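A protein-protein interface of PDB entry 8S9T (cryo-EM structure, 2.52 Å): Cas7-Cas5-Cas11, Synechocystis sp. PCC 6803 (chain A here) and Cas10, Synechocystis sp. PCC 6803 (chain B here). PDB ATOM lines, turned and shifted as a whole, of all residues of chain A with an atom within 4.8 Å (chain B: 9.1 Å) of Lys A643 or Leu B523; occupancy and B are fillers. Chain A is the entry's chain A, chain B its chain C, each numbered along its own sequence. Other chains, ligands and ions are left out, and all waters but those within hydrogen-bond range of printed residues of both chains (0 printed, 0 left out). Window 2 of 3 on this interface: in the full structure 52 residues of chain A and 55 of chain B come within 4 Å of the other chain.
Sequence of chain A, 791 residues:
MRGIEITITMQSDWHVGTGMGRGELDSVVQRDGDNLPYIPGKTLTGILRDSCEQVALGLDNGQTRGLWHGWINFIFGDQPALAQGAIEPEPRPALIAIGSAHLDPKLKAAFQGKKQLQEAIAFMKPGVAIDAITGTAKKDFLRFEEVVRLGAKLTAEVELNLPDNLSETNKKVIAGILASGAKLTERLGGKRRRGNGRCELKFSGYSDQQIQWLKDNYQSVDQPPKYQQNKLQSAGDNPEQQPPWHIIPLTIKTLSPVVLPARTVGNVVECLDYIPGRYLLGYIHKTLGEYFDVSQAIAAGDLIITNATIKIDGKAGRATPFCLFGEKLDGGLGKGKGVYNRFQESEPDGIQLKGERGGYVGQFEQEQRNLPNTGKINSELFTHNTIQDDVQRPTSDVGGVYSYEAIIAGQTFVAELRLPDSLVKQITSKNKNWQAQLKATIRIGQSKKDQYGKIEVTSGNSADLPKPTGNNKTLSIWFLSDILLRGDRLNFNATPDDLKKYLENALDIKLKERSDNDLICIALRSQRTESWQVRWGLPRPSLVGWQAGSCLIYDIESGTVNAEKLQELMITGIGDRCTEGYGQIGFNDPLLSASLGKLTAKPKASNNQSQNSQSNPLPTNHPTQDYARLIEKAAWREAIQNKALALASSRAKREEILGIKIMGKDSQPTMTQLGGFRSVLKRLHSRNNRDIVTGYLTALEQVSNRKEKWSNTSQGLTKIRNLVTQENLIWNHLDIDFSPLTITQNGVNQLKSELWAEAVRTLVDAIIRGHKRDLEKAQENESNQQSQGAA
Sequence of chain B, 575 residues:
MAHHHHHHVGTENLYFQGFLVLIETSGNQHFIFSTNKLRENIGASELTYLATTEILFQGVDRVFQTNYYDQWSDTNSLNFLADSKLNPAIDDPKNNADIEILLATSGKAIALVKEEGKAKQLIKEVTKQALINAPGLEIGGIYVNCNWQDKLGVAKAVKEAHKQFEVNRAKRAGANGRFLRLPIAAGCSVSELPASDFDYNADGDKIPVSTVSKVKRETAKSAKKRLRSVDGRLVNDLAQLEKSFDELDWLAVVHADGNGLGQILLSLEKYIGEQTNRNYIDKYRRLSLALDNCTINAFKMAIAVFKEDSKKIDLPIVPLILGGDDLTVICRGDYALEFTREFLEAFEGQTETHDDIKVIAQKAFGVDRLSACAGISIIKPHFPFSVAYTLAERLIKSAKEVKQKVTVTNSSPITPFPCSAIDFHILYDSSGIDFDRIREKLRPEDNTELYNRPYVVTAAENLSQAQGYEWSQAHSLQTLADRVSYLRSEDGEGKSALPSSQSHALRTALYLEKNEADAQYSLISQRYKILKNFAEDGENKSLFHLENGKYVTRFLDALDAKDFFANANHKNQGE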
ATOM      1  N   ALA A 639      -4.315  16.676  -7.275  1.00  0.00           N
ATOM      2  CA  ALA A 639      -5.018  17.908  -6.937  1.00  0.00           C
ATOM      3  C   ALA A 639      -6.460  17.880  -7.421  1.00  0.00           C
ATOM      4  O   ALA A 639      -7.380  18.217  -6.671  1.00  0.00           O
ATOM      5  CB  ALA A 639      -4.283  19.104  -7.530  1.00  0.00           C
ATOM      6  N   ILE A 640      -6.671  17.494  -8.681  1.00  0.00           N
ATOM      7  CA  ILE A 640      -8.019  17.415  -9.242  1.00  0.00           C
ATOM      8  C   ILE A 640      -8.886  16.456  -8.439  1.00  0.00           C
ATOM      9  O   ILE A 640      -9.995  16.798  -8.021  1.00  0.00           O
ATOM     10  CB  ILE A 640      -7.962  17.018 -10.729  1.00  0.00           C
ATOM     11  CG1 ILE A 640      -7.359  18.143 -11.568  1.00  0.00           C
ATOM     12  CG2 ILE A 640      -9.330  16.682 -11.248  1.00  0.00           C
ATOM     13  CD1 ILE A 640      -6.809  17.694 -12.897  1.00  0.00           C
ATOM     14  N   GLN A 641      -8.390  15.242  -8.210  1.00  0.00           N
ATOM     15  CA  GLN A 641      -9.163  14.230  -7.499  1.00  0.00           C
ATOM     16  C   GLN A 641      -9.492  14.649  -6.072  1.00  0.00           C
ATOM     17  O   GLN A 641     -10.604  14.406  -5.597  1.00  0.00           O
ATOM     18  CB  GLN A 641      -8.402  12.911  -7.504  1.00  0.00           C
ATOM     19  CG  GLN A 641      -8.307  12.276  -8.874  1.00  0.00           C
ATOM     20  CD  GLN A 641      -7.346  11.113  -8.909  1.00  0.00           C
ATOM     21  OE1 GLN A 641      -6.539  10.982  -9.829  1.00  0.00           O
ATOM     22  NE2 GLN A 641      -7.425  10.258  -7.899  1.00  0.00           N
ATOM     23  N   ASN A 642      -8.539  15.241  -5.358  1.00  0.00           N
ATOM     24  CA  ASN A 642      -8.820  15.705  -4.002  1.00  0.00           C
ATOM     25  C   ASN A 642      -9.839  16.836  -3.989  1.00  0.00           C
ATOM     26  O   ASN A 642     -10.784  16.821  -3.196  1.00  0.00           O
ATOM     27  CB  ASN A 642      -7.530  16.137  -3.309  1.00  0.00           C
ATOM     28  CG  ASN A 642      -6.648  14.965  -2.955  1.00  0.00           C
ATOM     29  OD1 ASN A 642      -7.098  13.818  -2.943  1.00  0.00           O
ATOM     30  ND2 ASN A 642      -5.382  15.241  -2.664  1.00  0.00           N
ATOM     31  N   LYS A 643      -9.656  17.833  -4.853  1.00  0.00           N
ATOM     32  CA  LYS A 643     -10.600  18.942  -4.929  1.00  0.00           C
ATOM     33  C   LYS A 643     -11.977  18.481  -5.389  1.00  0.00           C
ATOM     34  O   LYS A 643     -12.996  18.993  -4.915  1.00  0.00           O
ATOM     35  CB  LYS A 643     -10.053  20.022  -5.860  1.00  0.00           C
ATOM     36  CG  LYS A 643     -10.949  21.221  -6.016  1.00  0.00           C
ATOM     37  CD  LYS A 643     -11.277  21.859  -4.690  1.00  0.00           C
ATOM     38  CE  LYS A 643     -12.089  23.121  -4.896  1.00  0.00           C
ATOM     39  NZ  LYS A 643     -12.452  23.788  -3.619  1.00  0.00           N
ATOM     40  N   ALA A 644     -12.030  17.537  -6.327  1.00  0.00           N
ATOM     41  CA  ALA A 644     -13.307  16.950  -6.709  1.00  0.00           C
ATOM     42  C   ALA A 644     -14.006  16.314  -5.516  1.00  0.00           C
ATOM     43  O   ALA A 644     -15.196  16.540  -5.286  1.00  0.00           O
ATOM     44  CB  ALA A 644     -13.100  15.926  -7.823  1.00  0.00           C
ATOM     45  N   LEU A 645     -13.273  15.531  -4.731  1.00  0.00           N
ATOM     46  CA  LEU A 645     -13.872  14.849  -3.593  1.00  0.00           C
ATOM     47  C   LEU A 645     -14.278  15.803  -2.480  1.00  0.00           C
ATOM     48  O   LEU A 645     -15.211  15.508  -1.729  1.00  0.00           O
ATOM     49  CB  LEU A 645     -12.901  13.799  -3.072  1.00  0.00           C
ATOM     50  CG  LEU A 645     -12.770  12.595  -3.999  1.00  0.00           C
ATOM     51  CD1 LEU A 645     -11.520  11.835  -3.679  1.00  0.00           C
ATOM     52  CD2 LEU A 645     -13.965  11.697  -3.844  1.00  0.00           C
ATOM     53  N   ALA A 646     -13.589  16.932  -2.337  1.00  0.00           N
ATOM     54  CA  ALA A 646     -14.079  17.991  -1.464  1.00  0.00           C
ATOM     55  C   ALA A 646     -15.399  18.565  -1.964  1.00  0.00           C
ATOM     56  O   ALA A 646     -16.377  18.645  -1.215  1.00  0.00           O
ATOM     57  CB  ALA A 646     -13.027  19.086  -1.340  1.00  0.00           C
ATOM     58  N   LEU A 647     -15.435  18.992  -3.228  1.00  0.00           N
ATOM     59  CA  LEU A 647     -16.652  19.557  -3.807  1.00  0.00           C
ATOM     60  C   LEU A 647     -17.834  18.606  -3.690  1.00  0.00           C
ATOM     61  O   LEU A 647     -18.909  18.983  -3.214  1.00  0.00           O
ATOM     62  CB  LEU A 647     -16.416  19.912  -5.273  1.00  0.00           C
ATOM     63  CG  LEU A 647     -15.542  21.114  -5.618  1.00  0.00           C
ATOM     64  CD1 LEU A 647     -15.202  21.090  -7.089  1.00  0.00           C
ATOM     65  CD2 LEU A 647     -16.221  22.406  -5.241  1.00  0.00           C
ATOM     66  N   HIS A 733     -14.664  25.437 -11.949  1.00  0.00           N
ATOM     67  CA  HIS A 733     -15.269  24.732 -10.821  1.00  0.00           C
ATOM     68  C   HIS A 733     -14.217  24.154  -9.888  1.00  0.00           C
ATOM     69  O   HIS A 733     -14.342  24.260  -8.664  1.00  0.00           O
ATOM     70  CB  HIS A 733     -16.180  23.613 -11.319  1.00  0.00           C
ATOM     71  CG  HIS A 733     -17.493  24.090 -11.848  1.00  0.00           C
ATOM     72  ND1 HIS A 733     -18.369  24.838 -11.095  1.00  0.00           N
ATOM     73  CD2 HIS A 733     -18.083  23.916 -13.053  1.00  0.00           C
ATOM     74  CE1 HIS A 733     -19.441  25.110 -11.814  1.00  0.00           C
ATOM     75  NE2 HIS A 733     -19.291  24.563 -13.007  1.00  0.00           N
ATOM     76  N   LEU A 734     -13.180  23.532 -10.448  1.00  0.00           N
ATOM     77  CA  LEU A 734     -12.101  23.006  -9.627  1.00  0.00           C
ATOM     78  C   LEU A 734     -11.351  24.129  -8.929  1.00  0.00           C
ATOM     79  O   LEU A 734     -11.021  24.017  -7.745  1.00  0.00           O
ATOM     80  CB  LEU A 734     -11.168  22.169 -10.493  1.00  0.00           C
ATOM     81  CG  LEU A 734     -11.808  20.886 -11.035  1.00  0.00           C
ATOM     82  CD1 LEU A 734     -10.915  20.202 -12.047  1.00  0.00           C
ATOM     83  CD2 LEU A 734     -12.166  19.937  -9.907  1.00  0.00           C
ATOM     84  N   ILE A 736      -8.408  25.186  -8.955  1.00  0.00           N
ATOM     85  CA  ILE A 736      -7.066  24.867  -8.483  1.00  0.00           C
ATOM     86  C   ILE A 736      -6.078  25.865  -9.075  1.00  0.00           C
ATOM     87  O   ILE A 736      -6.127  26.163 -10.271  1.00  0.00           O
ATOM     88  CB  ILE A 736      -6.690  23.428  -8.852  1.00  0.00           C
ATOM     89  CG1 ILE A 736      -7.680  22.451  -8.229  1.00  0.00           C
ATOM     90  CG2 ILE A 736      -5.289  23.112  -8.343  1.00  0.00           C
ATOM     91  CD1 ILE A 736      -7.768  21.139  -8.945  1.00  0.00           C
ATOM     92  N   GLN B 502      -4.215  10.724   3.275  1.00  0.00           N
ATOM     93  CA  GLN B 502      -4.659  12.052   3.678  1.00  0.00           C
ATOM     94  C   GLN B 502      -3.772  12.659   4.746  1.00  0.00           C
ATOM     95  O   GLN B 502      -3.537  13.868   4.736  1.00  0.00           O
ATOM     96  CB  GLN B 502      -6.104  11.988   4.164  1.00  0.00           C
ATOM     97  CG  GLN B 502      -7.024  11.377   3.146  1.00  0.00           C
ATOM     98  CD  GLN B 502      -6.815  11.946   1.763  1.00  0.00           C
ATOM     99  OE1 GLN B 502      -6.583  13.139   1.592  1.00  0.00           O
ATOM    100  NE2 GLN B 502      -6.878  11.084   0.763  1.00  0.00           N
ATOM    101  N   ALA B 505      -0.831  14.009   2.820  1.00  0.00           N
ATOM    102  CA  ALA B 505      -1.209  15.262   2.170  1.00  0.00           C
ATOM    103  C   ALA B 505      -1.249  16.430   3.148  1.00  0.00           C
ATOM    104  O   ALA B 505      -0.918  17.562   2.785  1.00  0.00           O
ATOM    105  CB  ALA B 505      -2.559  15.102   1.486  1.00  0.00           C
ATOM    106  N   LEU B 506      -1.682  16.183   4.382  1.00  0.00           N
ATOM    107  CA  LEU B 506      -1.677  17.224   5.403  1.00  0.00           C
ATOM    108  C   LEU B 506      -0.273  17.566   5.876  1.00  0.00           C
ATOM    109  O   LEU B 506       0.023  18.735   6.137  1.00  0.00           O
ATOM    110  CB  LEU B 506      -2.550  16.789   6.571  1.00  0.00           C
ATOM    111  CG  LEU B 506      -4.046  16.823   6.293  1.00  0.00           C
ATOM    112  CD1 LEU B 506      -4.798  16.188   7.411  1.00  0.00           C
ATOM    113  CD2 LEU B 506      -4.483  18.259   6.128  1.00  0.00           C
ATOM    114  N   ALA B 509       0.838  19.828   3.169  1.00  0.00           N
ATOM    115  CA  ALA B 509       0.167  21.119   3.265  1.00  0.00           C
ATOM    116  C   ALA B 509       0.778  22.011   4.337  1.00  0.00           C
ATOM    117  O   ALA B 509       0.874  23.226   4.157  1.00  0.00           O
ATOM    118  CB  ALA B 509      -1.318  20.914   3.538  1.00  0.00           C
ATOM    119  N   ASN B 515      -2.238  30.164   3.833  1.00  0.00           N
ATOM    120  CA  ASN B 515      -3.470  30.108   3.062  1.00  0.00           C
ATOM    121  C   ASN B 515      -3.546  28.852   2.204  1.00  0.00           C
ATOM    122  O   ASN B 515      -4.638  28.330   1.976  1.00  0.00           O
ATOM    123  CB  ASN B 515      -3.609  31.366   2.213  1.00  0.00           C
ATOM    124  CG  ASN B 515      -3.831  32.600   3.054  1.00  0.00           C
ATOM    125  OD1 ASN B 515      -3.855  32.531   4.281  1.00  0.00           O
ATOM    126  ND2 ASN B 515      -4.008  33.740   2.400  1.00  0.00           N
ATOM    127  N   GLU B 516      -2.409  28.361   1.707  1.00  0.00           N
ATOM    128  CA  GLU B 516      -2.409  27.075   1.017  1.00  0.00           C
ATOM    129  C   GLU B 516      -2.578  25.927   2.002  1.00  0.00           C
ATOM    130  O   GLU B 516      -3.275  24.950   1.712  1.00  0.00           O
ATOM    131  CB  GLU B 516      -1.125  26.897   0.212  1.00  0.00           C
ATOM    132  CG  GLU B 516      -0.876  27.963  -0.824  1.00  0.00           C
ATOM    133  CD  GLU B 516       0.411  27.731  -1.597  1.00  0.00           C
ATOM    134  OE1 GLU B 516       1.452  27.438  -0.971  1.00  0.00           O
ATOM    135  OE2 GLU B 516       0.380  27.841  -2.843  1.00  0.00           O
ATOM    136  N   ALA B 517      -1.922  26.014   3.159  1.00  0.00           N
ATOM    137  CA  ALA B 517      -2.100  25.006   4.196  1.00  0.00           C
ATOM    138  C   ALA B 517      -3.539  24.958   4.689  1.00  0.00           C
ATOM    139  O   ALA B 517      -4.121  23.878   4.836  1.00  0.00           O
ATOM    140  CB  ALA B 517      -1.143  25.279   5.351  1.00  0.00           C
ATOM    141  N   ASP B 518      -4.132  26.122   4.955  1.00  0.00           N
ATOM    142  CA  ASP B 518      -5.525  26.168   5.391  1.00  0.00           C
ATOM    143  C   ASP B 518      -6.499  25.775   4.289  1.00  0.00           C
ATOM    144  O   ASP B 518      -7.538  25.179   4.576  1.00  0.00           O
ATOM    145  CB  ASP B 518      -5.863  27.560   5.913  1.00  0.00           C
ATOM    146  CG  ASP B 518      -5.191  27.867   7.225  1.00  0.00           C
ATOM    147  OD1 ASP B 518      -4.670  26.930   7.861  1.00  0.00           O
ATOM    148  OD2 ASP B 518      -5.186  29.047   7.630  1.00  0.00           O
ATOM    149  N   ALA B 519      -6.194  26.099   3.032  1.00  0.00           N
ATOM    150  CA  ALA B 519      -7.025  25.639   1.925  1.00  0.00           C
ATOM    151  C   ALA B 519      -7.048  24.121   1.841  1.00  0.00           C
ATOM    152  O   ALA B 519      -8.110  23.514   1.688  1.00  0.00           O
ATOM    153  CB  ALA B 519      -6.528  26.237   0.613  1.00  0.00           C
ATOM    154  N   GLN B 520      -5.873  23.498   1.896  1.00  0.00           N
ATOM    155  CA  GLN B 520      -5.783  22.043   1.916  1.00  0.00           C
ATOM    156  C   GLN B 520      -6.517  21.443   3.105  1.00  0.00           C
ATOM    157  O   GLN B 520      -7.224  20.441   2.963  1.00  0.00           O
ATOM    158  CB  GLN B 520      -4.319  21.623   1.934  1.00  0.00           C
ATOM    159  CG  GLN B 520      -3.576  21.824   0.640  1.00  0.00           C
ATOM    160  CD  GLN B 520      -4.031  20.875  -0.435  1.00  0.00           C
ATOM    161  OE1 GLN B 520      -4.567  21.290  -1.459  1.00  0.00           O
ATOM    162  NE2 GLN B 520      -3.827  19.585  -0.204  1.00  0.00           N
ATOM    163  N   TYR B 521      -6.339  22.023   4.290  1.00  0.00           N
ATOM    164  CA  TYR B 521      -7.069  21.562   5.466  1.00  0.00           C
ATOM    165  C   TYR B 521      -8.579  21.653   5.282  1.00  0.00           C
ATOM    166  O   TYR B 521      -9.317  20.801   5.779  1.00  0.00           O
ATOM    167  CB  TYR B 521      -6.631  22.349   6.705  1.00  0.00           C
ATOM    168  CG  TYR B 521      -7.542  22.112   7.877  1.00  0.00           C
ATOM    169  CD1 TYR B 521      -7.584  20.887   8.512  1.00  0.00           C
ATOM    170  CD2 TYR B 521      -8.401  23.103   8.315  1.00  0.00           C
ATOM    171  CE1 TYR B 521      -8.419  20.672   9.570  1.00  0.00           C
ATOM    172  CE2 TYR B 521      -9.257  22.886   9.359  1.00  0.00           C
ATOM    173  CZ  TYR B 521      -9.254  21.673   9.988  1.00  0.00           C
ATOM    174  OH  TYR B 521     -10.111  21.448  11.028  1.00  0.00           O
ATOM    175  N   SER B 522      -9.062  22.693   4.605  1.00  0.00           N
ATOM    176  CA  SER B 522     -10.492  22.777   4.320  1.00  0.00           C
ATOM    177  C   SER B 522     -10.952  21.640   3.419  1.00  0.00           C
ATOM    178  O   SER B 522     -11.951  20.973   3.702  1.00  0.00           O
ATOM    179  CB  SER B 522     -10.825  24.124   3.685  1.00  0.00           C
ATOM    180  OG  SER B 522     -10.459  25.188   4.537  1.00  0.00           O
ATOM    181  N   LEU B 523     -10.239  21.419   2.315  1.00  0.00           N
ATOM    182  CA  LEU B 523     -10.589  20.351   1.383  1.00  0.00           C
ATOM    183  C   LEU B 523     -10.618  18.986   2.053  1.00  0.00           C
ATOM    184  O   LEU B 523     -11.548  18.202   1.840  1.00  0.00           O
ATOM    185  CB  LEU B 523      -9.622  20.354   0.206  1.00  0.00           C
ATOM    186  CG  LEU B 523     -10.023  21.172  -1.016  1.00  0.00           C
ATOM    187  CD1 LEU B 523     -10.676  22.481  -0.633  1.00  0.00           C
ATOM    188  CD2 LEU B 523      -8.796  21.418  -1.868  1.00  0.00           C
ATOM    189  N   ILE B 524      -9.601  18.671   2.849  1.00  0.00           N
ATOM    190  CA  ILE B 524      -9.530  17.332   3.422  1.00  0.00           C
ATOM    191  C   ILE B 524     -10.519  17.167   4.570  1.00  0.00           C
ATOM    192  O   ILE B 524     -11.087  16.091   4.757  1.00  0.00           O
ATOM    193  CB  ILE B 524      -8.085  17.001   3.837  1.00  0.00           C
ATOM    194  CG1 ILE B 524      -7.162  17.121   2.627  1.00  0.00           C
ATOM    195  CG2 ILE B 524      -7.994  15.594   4.373  1.00  0.00           C
ATOM    196  CD1 ILE B 524      -5.695  17.117   2.951  1.00  0.00           C
ATOM    197  N   SER B 525     -10.747  18.217   5.355  1.00  0.00           N
ATOM    198  CA  SER B 525     -11.711  18.114   6.442  1.00  0.00           C
ATOM    199  C   SER B 525     -13.158  18.122   5.966  1.00  0.00           C
ATOM    200  O   SER B 525     -14.027  17.641   6.694  1.00  0.00           O
ATOM    201  CB  SER B 525     -11.472  19.225   7.464  1.00  0.00           C
ATOM    202  OG  SER B 525     -11.652  20.501   6.894  1.00  0.00           O
ATOM    203  N   GLN B 526     -13.442  18.643   4.771  1.00  0.00           N
ATOM    204  CA  GLN B 526     -14.759  18.423   4.175  1.00  0.00           C
ATOM    205  C   GLN B 526     -15.011  16.943   3.939  1.00  0.00           C
ATOM    206  O   GLN B 526     -16.127  16.449   4.135  1.00  0.00           O
ATOM    207  CB  GLN B 526     -14.883  19.183   2.856  1.00  0.00           C
ATOM    208  CG  GLN B 526     -15.096  20.673   2.995  1.00  0.00           C
ATOM    209  CD  GLN B 526     -14.819  21.420   1.705  1.00  0.00           C
ATOM    210  OE1 GLN B 526     -14.995  20.885   0.619  1.00  0.00           O
ATOM    211  NE2 GLN B 526     -14.363  22.657   1.822  1.00  0.00           N
ATOM    212  N   ARG B 527     -13.983  16.225   3.522  1.00  0.00           N
ATOM    213  CA  ARG B 527     -14.055  14.816   3.180  1.00  0.00           C
ATOM    214  C   ARG B 527     -13.892  13.884   4.376  1.00  0.00           C
ATOM    215  O   ARG B 527     -14.481  12.799   4.383  1.00  0.00           O
ATOM    216  CB  ARG B 527     -12.988  14.515   2.136  1.00  0.00           C
ATOM    217  CG  ARG B 527     -13.065  13.167   1.514  1.00  0.00           C
ATOM    218  CD  ARG B 527     -11.903  13.024   0.574  1.00  0.00           C
ATOM    219  NE  ARG B 527     -11.687  11.645   0.163  1.00  0.00           N
ATOM    220  CZ  ARG B 527     -10.646  11.262  -0.563  1.00  0.00           C
ATOM    221  NH1 ARG B 527      -9.750  12.164  -0.945  1.00  0.00           N
ATOM    222  NH2 ARG B 527     -10.501   9.990  -0.913  1.00  0.00           N
ATOM    223  N   TYR B 528     -13.106  14.268   5.382  1.00  0.00           N
ATOM    224  CA  TYR B 528     -12.816  13.426   6.548  1.00  0.00           C
ATOM    225  C   TYR B 528     -13.058  14.251   7.802  1.00  0.00           C
ATOM    226  O   TYR B 528     -12.144  14.890   8.323  1.00  0.00           O
ATOM    227  CB  TYR B 528     -11.390  12.907   6.500  1.00  0.00           C
ATOM    228  CG  TYR B 528     -11.180  11.884   5.430  1.00  0.00           C
ATOM    229  CD1 TYR B 528     -11.504  10.559   5.641  1.00  0.00           C
ATOM    230  CD2 TYR B 528     -10.690  12.251   4.192  1.00  0.00           C
ATOM    231  CE1 TYR B 528     -11.330   9.628   4.653  1.00  0.00           C
ATOM    232  CE2 TYR B 528     -10.519  11.329   3.203  1.00  0.00           C
ATOM    233  CZ  TYR B 528     -10.835  10.021   3.435  1.00  0.00           C
ATOM    234  OH  TYR B 528     -10.655   9.095   2.441  1.00  0.00           O
ATOM    235  N   LYS B 529     -14.295  14.211   8.291  1.00  0.00           N
ATOM    236  CA  LYS B 529     -14.768  15.168   9.281  1.00  0.00           C
ATOM    237  C   LYS B 529     -14.081  15.044  10.633  1.00  0.00           C
ATOM    238  O   LYS B 529     -14.206  15.958  11.450  1.00  0.00           O
ATOM    239  CB  LYS B 529     -16.280  15.039   9.427  1.00  0.00           C
ATOM    240  CG  LYS B 529     -17.012  15.472   8.165  1.00  0.00           C
ATOM    241  CD  LYS B 529     -17.015  16.984   8.032  1.00  0.00           C
ATOM    242  CE  LYS B 529     -17.779  17.435   6.806  1.00  0.00           C
ATOM    243  NZ  LYS B 529     -17.992  18.904   6.809  1.00  0.00           N
ATOM    244  N   LEU B 531     -11.096  15.485  11.174  1.00  0.00           N
ATOM    245  CA  LEU B 531     -10.124  16.570  11.229  1.00  0.00           C
ATOM    246  C   LEU B 531     -10.627  17.838  11.903  1.00  0.00           C
ATOM    247  O   LEU B 531      -9.807  18.690  12.254  1.00  0.00           O
ATOM    248  CB  LEU B 531      -9.648  16.925   9.829  1.00  0.00           C
ATOM    249  CG  LEU B 531      -8.603  15.978   9.280  1.00  0.00           C
ATOM    250  CD1 LEU B 531      -8.430  16.244   7.818  1.00  0.00           C
ATOM    251  CD2 LEU B 531      -7.311  16.171  10.041  1.00  0.00           C
ATOM    252  N   LYS B 541     -11.195  26.293  10.991  1.00  0.00           N
ATOM    253  CA  LYS B 541     -10.786  26.414   9.600  1.00  0.00           C
ATOM    254  C   LYS B 541      -9.272  26.422   9.409  1.00  0.00           C
ATOM    255  O   LYS B 541      -8.810  26.672   8.292  1.00  0.00           O
ATOM    256  CB  LYS B 541     -11.396  27.669   8.977  1.00  0.00           C
ATOM    257  CG  LYS B 541     -11.066  28.957   9.690  1.00  0.00           C
ATOM    258  CD  LYS B 541     -11.732  30.127   9.001  1.00  0.00           C
ATOM    259  CE  LYS B 541     -13.222  29.874   8.826  1.00  0.00           C
ATOM    260  NZ  LYS B 541     -13.965  29.933  10.113  1.00  0.00           N
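O of Ala A646 lies close to OE1 of Gln B526, 3.2 Å away.
Lys A643 touches just one residue of chain B: Leu B523. Of the printed residues of chain B, Leu A645 touches Arg B527. Of chain B, only Leu B523 and Gln B526 come within 4 Å of Ala A646. Leu B523 touches just these residues of chain A: Lys A643 (3.7 Å) and Ala A646 (3.6 Å). Of the printed residues of chain A, Arg B527 touches Asn A642 and Leu A645. The nearest residue of chain B that does not touch Lys A643 is Gln B526 (5.7 Å). The nearest printed residue of chain B that does not touch Leu A645 is Leu B523 (5.6 Å).
O of Ser B522 sits close to NE2 of Gln B526, at 3.5 Å. The side-chain hydroxyl (OH) of Tyr B528 is in hydrogen-bond range of the guanidinium group (NH2) of Arg B527, at 3.5 Å.
Arg B527 touches Asn A642 (NH1 to OD1, 3.7 Å). Lys A643 touches Leu B523. Leu A645 touches Arg B527. O of Leu B523 touches CB of Ala A646 (3.6 Å).
Hydrophobic or aromatic side chains of chain A that line the printed part of chain B: Leu A645 and Ala A646. Among the printed residues, 5 pairs touch across the chains. Among the printed residues, no Asp or Glu carboxylate lies within 4 Å of a Lys or Arg side-chain nitrogen of the other chain.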
